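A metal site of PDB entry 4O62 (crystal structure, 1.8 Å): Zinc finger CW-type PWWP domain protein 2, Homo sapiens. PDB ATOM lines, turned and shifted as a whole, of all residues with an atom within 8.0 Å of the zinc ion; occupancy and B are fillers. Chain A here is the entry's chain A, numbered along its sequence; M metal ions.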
ATOM      1  N   GLN A  13      29.494  25.905  -1.089  1.00  0.00           N
ATOM      2  CA  GLN A  13      28.910  24.686  -1.635  1.00  0.00           C
ATOM      3  C   GLN A  13      29.352  23.421  -0.870  1.00  0.00           C
ATOM      4  O   GLN A  13      30.542  23.193  -0.635  1.00  0.00           O
ATOM      5  CB  GLN A  13      29.286  24.563  -3.101  1.00  0.00           C
ATOM      6  CG  GLN A  13      28.413  23.567  -3.840  1.00  0.00           C
ATOM      7  CD  GLN A  13      28.827  23.412  -5.294  1.00  0.00           C
ATOM      8  OE1 GLN A  13      29.849  23.934  -5.723  1.00  0.00           O
ATOM      9  NE2 GLN A  13      27.998  22.723  -6.055  1.00  0.00           N
ATOM     10  N   CYS A  14      28.367  22.589  -0.528  1.00  0.00           N
ATOM     11  CA  CYS A  14      28.597  21.335   0.123  1.00  0.00           C
ATOM     12  C   CYS A  14      29.462  20.464  -0.787  1.00  0.00           C
ATOM     13  O   CYS A  14      29.279  20.439  -2.033  1.00  0.00           O
ATOM     14  CB  CYS A  14      27.280  20.639   0.393  1.00  0.00           C
ATOM     15  SG  CYS A  14      27.447  19.050   1.199  1.00  0.00           S
ATOM     16  N   GLU A  15      30.439  19.799  -0.166  1.00  0.00           N
ATOM     17  CA  GLU A  15      31.364  18.959  -0.914  1.00  0.00           C
ATOM     18  C   GLU A  15      30.995  17.493  -0.869  1.00  0.00           C
ATOM     19  O   GLU A  15      31.745  16.658  -1.372  1.00  0.00           O
ATOM     20  CB  GLU A  15      32.811  19.225  -0.473  1.00  0.00           C
ATOM     21  CG  GLU A  15      33.289  20.634  -0.865  1.00  0.00           C
ATOM     22  CD  GLU A  15      34.649  20.985  -0.317  1.00  0.00           C
ATOM     23  OE1 GLU A  15      35.582  20.220  -0.558  1.00  0.00           O
ATOM     24  OE2 GLU A  15      34.771  22.045   0.319  1.00  0.00           O
ATOM     25  N   ASN A  16      29.848  17.147  -0.262  1.00  0.00           N
ATOM     26  CA  ASN A  16      29.281  15.779  -0.420  1.00  0.00           C
ATOM     27  C   ASN A  16      28.832  15.667  -1.889  1.00  0.00           C
ATOM     28  O   ASN A  16      27.967  16.391  -2.338  1.00  0.00           O
ATOM     29  CB  ASN A  16      28.139  15.562   0.567  1.00  0.00           C
ATOM     30  CG  ASN A  16      27.411  14.250   0.386  1.00  0.00           C
ATOM     31  OD1 ASN A  16      27.827  13.376  -0.375  1.00  0.00           O
ATOM     32  ND2 ASN A  16      26.340  14.065   1.146  1.00  0.00           N
ATOM     33  N   GLU A  17      29.522  14.824  -2.651  1.00  0.00           N
ATOM     34  CA  GLU A  17      29.287  14.625  -4.087  1.00  0.00           C
ATOM     35  C   GLU A  17      27.840  14.180  -4.359  1.00  0.00           C
ATOM     36  O   GLU A  17      27.336  14.384  -5.462  1.00  0.00           O
ATOM     37  CB  GLU A  17      30.293  13.568  -4.672  1.00  0.00           C
ATOM     38  N   ASN A  18      27.167  13.578  -3.372  1.00  0.00           N
ATOM     39  CA  ASN A  18      25.752  13.233  -3.516  1.00  0.00           C
ATOM     40  C   ASN A  18      24.821  14.451  -3.379  1.00  0.00           C
ATOM     41  O   ASN A  18      23.647  14.355  -3.706  1.00  0.00           O
ATOM     42  CB  ASN A  18      25.312  12.252  -2.443  1.00  0.00           C
ATOM     43  CG  ASN A  18      25.910  10.877  -2.612  1.00  0.00           C
ATOM     44  OD1 ASN A  18      26.330  10.464  -3.705  1.00  0.00           O
ATOM     45  ND2 ASN A  18      25.916  10.146  -1.522  1.00  0.00           N
ATOM     46  N   CYS A  19      25.351  15.562  -2.852  1.00  0.00           N
ATOM     47  CA  CYS A  19      24.538  16.705  -2.449  1.00  0.00           C
ATOM     48  C   CYS A  19      24.853  17.922  -3.287  1.00  0.00           C
ATOM     49  O   CYS A  19      24.029  18.334  -4.094  1.00  0.00           O
ATOM     50  CB  CYS A  19      24.735  17.002  -0.958  1.00  0.00           C
ATOM     51  SG  CYS A  19      23.899  18.515  -0.362  1.00  0.00           S
ATOM     52  N   LEU A  20      26.038  18.526  -3.085  1.00  0.00           N
ATOM     53  CA  LEU A  20      26.464  19.699  -3.888  1.00  0.00           C
ATOM     54  C   LEU A  20      25.558  20.950  -3.782  1.00  0.00           C
ATOM     55  O   LEU A  20      25.648  21.849  -4.591  1.00  0.00           O
ATOM     56  CB  LEU A  20      26.651  19.316  -5.370  1.00  0.00           C
ATOM     57  CG  LEU A  20      27.656  18.155  -5.572  1.00  0.00           C
ATOM     58  CD1 LEU A  20      27.682  17.744  -7.036  1.00  0.00           C
ATOM     59  CD2 LEU A  20      29.062  18.548  -5.083  1.00  0.00           C
ATOM     60  N   LYS A  21      24.738  21.015  -2.724  1.00  0.00           N
ATOM     61  CA  LYS A  21      23.896  22.183  -2.492  1.00  0.00           C
ATOM     62  C   LYS A  21      24.707  23.402  -1.977  1.00  0.00           C
ATOM     63  O   LYS A  21      25.695  23.238  -1.278  1.00  0.00           O
ATOM     64  CB  LYS A  21      22.787  21.847  -1.500  1.00  0.00           C
ATOM     65  CG  LYS A  21      21.753  20.805  -2.009  1.00  0.00           C
ATOM     66  CD  LYS A  21      20.787  20.440  -0.895  1.00  0.00           C
ATOM     67  CE  LYS A  21      19.846  19.291  -1.214  1.00  0.00           C
ATOM     68  NZ  LYS A  21      20.556  18.011  -1.446  1.00  0.00           N
ATOM     69  N   TRP A  22      24.232  24.586  -2.318  1.00  0.00           N
ATOM     70  CA  TRP A  22      24.792  25.856  -1.888  1.00  0.00           C
ATOM     71  C   TRP A  22      24.063  26.359  -0.635  1.00  0.00           C
ATOM     72  O   TRP A  22      22.822  26.247  -0.510  1.00  0.00           O
ATOM     73  CB  TRP A  22      24.634  26.847  -2.996  1.00  0.00           C
ATOM     74  CG  TRP A  22      25.608  26.666  -4.101  1.00  0.00           C
ATOM     75  CD1 TRP A  22      25.428  25.909  -5.247  1.00  0.00           C
ATOM     76  CD2 TRP A  22      26.917  27.265  -4.205  1.00  0.00           C
ATOM     77  NE1 TRP A  22      26.540  26.038  -6.063  1.00  0.00           N
ATOM     78  CE2 TRP A  22      27.468  26.837  -5.446  1.00  0.00           C
ATOM     79  CE3 TRP A  22      27.659  28.129  -3.393  1.00  0.00           C
ATOM     80  CZ2 TRP A  22      28.735  27.237  -5.877  1.00  0.00           C
ATOM     81  CZ3 TRP A  22      28.939  28.541  -3.831  1.00  0.00           C
ATOM     82  CH2 TRP A  22      29.457  28.094  -5.086  1.00  0.00           C
ATOM     83  N   ARG A  23      24.852  26.930   0.278  1.00  0.00           N
ATOM     84  CA  ARG A  23      24.391  27.303   1.606  1.00  0.00           C
ATOM     85  C   ARG A  23      24.897  28.705   1.881  1.00  0.00           C
ATOM     86  O   ARG A  23      26.081  28.992   1.643  1.00  0.00           O
ATOM     87  CB  ARG A  23      24.934  26.367   2.683  1.00  0.00           C
ATOM     88  CG  ARG A  23      24.489  24.902   2.593  1.00  0.00           C
ATOM     89  CD  ARG A  23      22.991  24.752   2.465  1.00  0.00           C
ATOM     90  NE  ARG A  23      22.582  23.340   2.510  1.00  0.00           N
ATOM     91  CZ  ARG A  23      21.347  22.897   2.264  1.00  0.00           C
ATOM     92  NH1 ARG A  23      20.370  23.753   1.961  1.00  0.00           N
ATOM     93  NH2 ARG A  23      21.086  21.571   2.372  1.00  0.00           N
ATOM     94  N   TRP A  39      34.031  21.397   3.237  1.00  0.00           N
ATOM     95  CA  TRP A  39      32.854  21.916   3.908  1.00  0.00           C
ATOM     96  C   TRP A  39      31.625  21.125   3.453  1.00  0.00           C
ATOM     97  O   TRP A  39      31.497  20.811   2.272  1.00  0.00           O
ATOM     98  CB  TRP A  39      32.677  23.406   3.586  1.00  0.00           C
ATOM     99  CG  TRP A  39      31.651  24.018   4.479  1.00  0.00           C
ATOM    100  CD1 TRP A  39      31.898  24.655   5.692  1.00  0.00           C
ATOM    101  CD2 TRP A  39      30.230  24.048   4.293  1.00  0.00           C
ATOM    102  NE1 TRP A  39      30.710  25.068   6.262  1.00  0.00           N
ATOM    103  CE2 TRP A  39      29.674  24.701   5.441  1.00  0.00           C
ATOM    104  CE3 TRP A  39      29.355  23.572   3.291  1.00  0.00           C
ATOM    105  CZ2 TRP A  39      28.309  24.924   5.598  1.00  0.00           C
ATOM    106  CZ3 TRP A  39      27.962  23.793   3.447  1.00  0.00           C
ATOM    107  CH2 TRP A  39      27.456  24.445   4.599  1.00  0.00           C
ATOM    108  N   TYR A  40      30.756  20.808   4.415  1.00  0.00           N
ATOM    109  CA  TYR A  40      29.541  19.992   4.212  1.00  0.00           C
ATOM    110  C   TYR A  40      28.400  20.643   4.968  1.00  0.00           C
ATOM    111  O   TYR A  40      28.601  21.340   5.963  1.00  0.00           O
ATOM    112  CB  TYR A  40      29.744  18.585   4.755  1.00  0.00           C
ATOM    113  CG  TYR A  40      30.967  17.865   4.212  1.00  0.00           C
ATOM    114  CD1 TYR A  40      31.016  17.424   2.898  1.00  0.00           C
ATOM    115  CD2 TYR A  40      32.074  17.618   5.030  1.00  0.00           C
ATOM    116  CE1 TYR A  40      32.134  16.757   2.399  1.00  0.00           C
ATOM    117  CE2 TYR A  40      33.195  16.927   4.546  1.00  0.00           C
ATOM    118  CZ  TYR A  40      33.220  16.512   3.237  1.00  0.00           C
ATOM    119  OH  TYR A  40      34.294  15.858   2.738  1.00  0.00           O
ATOM    120  N   CYS A  41      27.192  20.323   4.529  1.00  0.00           N
ATOM    121  CA  CYS A  41      25.980  20.929   5.049  1.00  0.00           C
ATOM    122  C   CYS A  41      25.865  20.911   6.560  1.00  0.00           C
ATOM    123  O   CYS A  41      25.397  21.905   7.173  1.00  0.00           O
ATOM    124  CB  CYS A  41      24.725  20.208   4.455  1.00  0.00           C
ATOM    125  SG  CYS A  41      24.385  20.637   2.740  1.00  0.00           S
ATOM    126  N   PHE A  42      26.267  19.792   7.163  1.00  0.00           N
ATOM    127  CA  PHE A  42      26.090  19.610   8.594  1.00  0.00           C
ATOM    128  C   PHE A  42      26.927  20.597   9.419  1.00  0.00           C
ATOM    129  O   PHE A  42      26.702  20.733  10.603  1.00  0.00           O
ATOM    130  CB  PHE A  42      26.375  18.168   9.059  1.00  0.00           C
ATOM    131  CG  PHE A  42      27.820  17.756   8.977  1.00  0.00           C
ATOM    132  CD1 PHE A  42      28.664  17.939  10.076  1.00  0.00           C
ATOM    133  CD2 PHE A  42      28.330  17.139   7.839  1.00  0.00           C
ATOM    134  CE1 PHE A  42      29.988  17.537  10.015  1.00  0.00           C
ATOM    135  CE2 PHE A  42      29.660  16.744   7.774  1.00  0.00           C
ATOM    136  CZ  PHE A  42      30.488  16.954   8.867  1.00  0.00           C
ATOM    137  N   TYR A  49      18.946  24.969   7.367  1.00  0.00           N
ATOM    138  CA  TYR A  49      19.612  24.524   6.109  1.00  0.00           C
ATOM    139  C   TYR A  49      20.884  23.714   6.391  1.00  0.00           C
ATOM    140  O   TYR A  49      21.857  23.808   5.646  1.00  0.00           O
ATOM    141  CB  TYR A  49      19.922  25.734   5.193  1.00  0.00           C
ATOM    142  CG  TYR A  49      18.681  26.471   4.722  1.00  0.00           C
ATOM    143  CD1 TYR A  49      17.820  25.911   3.784  1.00  0.00           C
ATOM    144  CD2 TYR A  49      18.353  27.730   5.216  1.00  0.00           C
ATOM    145  CE1 TYR A  49      16.671  26.555   3.366  1.00  0.00           C
ATOM    146  CE2 TYR A  49      17.223  28.398   4.796  1.00  0.00           C
ATOM    147  CZ  TYR A  49      16.386  27.806   3.868  1.00  0.00           C
ATOM    148  OH  TYR A  49      15.248  28.416   3.436  1.00  0.00           O
ATOM    149  N   ASN A  50      20.878  22.958   7.495  1.00  0.00           N
ATOM    150  CA  ASN A  50      22.108  22.345   8.006  1.00  0.00           C
ATOM    151  C   ASN A  50      22.172  20.838   7.766  1.00  0.00           C
ATOM    152  O   ASN A  50      22.700  20.100   8.600  1.00  0.00           O
ATOM    153  CB  ASN A  50      22.250  22.618   9.520  1.00  0.00           C
ATOM    154  CG  ASN A  50      21.082  22.021  10.316  1.00  0.00           C
ATOM    155  OD1 ASN A  50      20.081  21.548   9.751  1.00  0.00           O
ATOM    156  ND2 ASN A  50      21.216  22.032  11.614  1.00  0.00           N
ATOM    157  N   ASN A  51      21.583  20.354   6.658  1.00  0.00           N
ATOM    158  CA  ASN A  51      21.625  18.941   6.357  1.00  0.00           C
ATOM    159  C   ASN A  51      21.474  18.767   4.841  1.00  0.00           C
ATOM    160  O   ASN A  51      20.723  19.513   4.198  1.00  0.00           O
ATOM    161  CB  ASN A  51      20.571  18.191   7.162  1.00  0.00           C
ATOM    162  CG  ASN A  51      20.864  16.696   7.271  1.00  0.00           C
ATOM    163  OD1 ASN A  51      20.590  15.935   6.357  1.00  0.00           O
ATOM    164  ND2 ASN A  51      21.444  16.278   8.394  1.00  0.00           N
ATOM    165  N   CYS A  52      22.235  17.819   4.290  1.00  0.00           N
ATOM    166  CA  CYS A  52      22.197  17.487   2.855  1.00  0.00           C
ATOM    167  C   CYS A  52      20.794  17.123   2.372  1.00  0.00           C
ATOM    168  O   CYS A  52      20.471  17.307   1.199  1.00  0.00           O
ATOM    169  CB  CYS A  52      23.179  16.347   2.568  1.00  0.00           C
ATOM    170  SG  CYS A  52      24.945  16.730   2.806  1.00  0.00           S
ATOM    171  N   SER A  53      19.950  16.626   3.270  1.00  0.00           N
ATOM    172  CA  SER A  53      18.585  16.218   2.911  1.00  0.00           C
ATOM    173  C   SER A  53      17.617  17.410   2.824  1.00  0.00           C
ATOM    174  O   SER A  53      16.514  17.259   2.359  1.00  0.00           O
ATOM    175  CB  SER A  53      18.089  15.172   3.901  1.00  0.00           C
ATOM    176  OG  SER A  53      17.806  15.770   5.137  1.00  0.00           O
ATOM    177  N   ILE A  54      18.056  18.594   3.241  1.00  0.00           N
ATOM    178  CA  ILE A  54      17.262  19.814   3.162  1.00  0.00           C
ATOM    179  C   ILE A  54      17.513  20.565   1.854  1.00  0.00           C
ATOM    180  O   ILE A  54      18.670  20.766   1.467  1.00  0.00           O
ATOM    181  CB  ILE A  54      17.545  20.757   4.364  1.00  0.00           C
ATOM    182  CG1 ILE A  54      17.265  20.014   5.689  1.00  0.00           C
ATOM    183  CG2 ILE A  54      16.697  22.025   4.275  1.00  0.00           C
ATOM    184  CD1 ILE A  54      17.849  20.693   6.922  1.00  0.00           C
HETATM  185 ZN    ZN M   1      25.184  18.747   1.585  1.00  0.00          ZN
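N of Asn 16 sits close to SG of Cys 14 (3.4 Å). The backbone NH of Cys 14 lies within hydrogen-bond range of the backbone carbonyl oxygen of Lys 21 (2.9 Å). SG of Cys 19 sits close to N of Lys 21, at 3.5 Å. The side-chain sulfur (SG) of Cys 41 lies close to the guanidinium group (NE) of Arg 23 (3.3 Å). The side-chain amide nitrogen (ND2) of Asn 16 sits close to the side-chain sulfur (SG) of Cys 52 (3.4 Å). O of Cys 52 sits at hydrogen-bond distance from NZ of Lys 21, 2.7 Å away.
Of the 21 residues printed, 4 come within 4 Å of the zinc ion. The nearest printed residue that does not touch the zinc ion is Asn 16 (4.5 Å).
The zinc ion is bound by the side-chain sulfur (SG) of Cys 14. SG of Cys 19 binds the zinc ion (2.3 Å). The side-chain sulfur (SG) of Cys 41 binds the zinc ion. SG of Cys 52 binds the zinc ion (2.4 Å).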
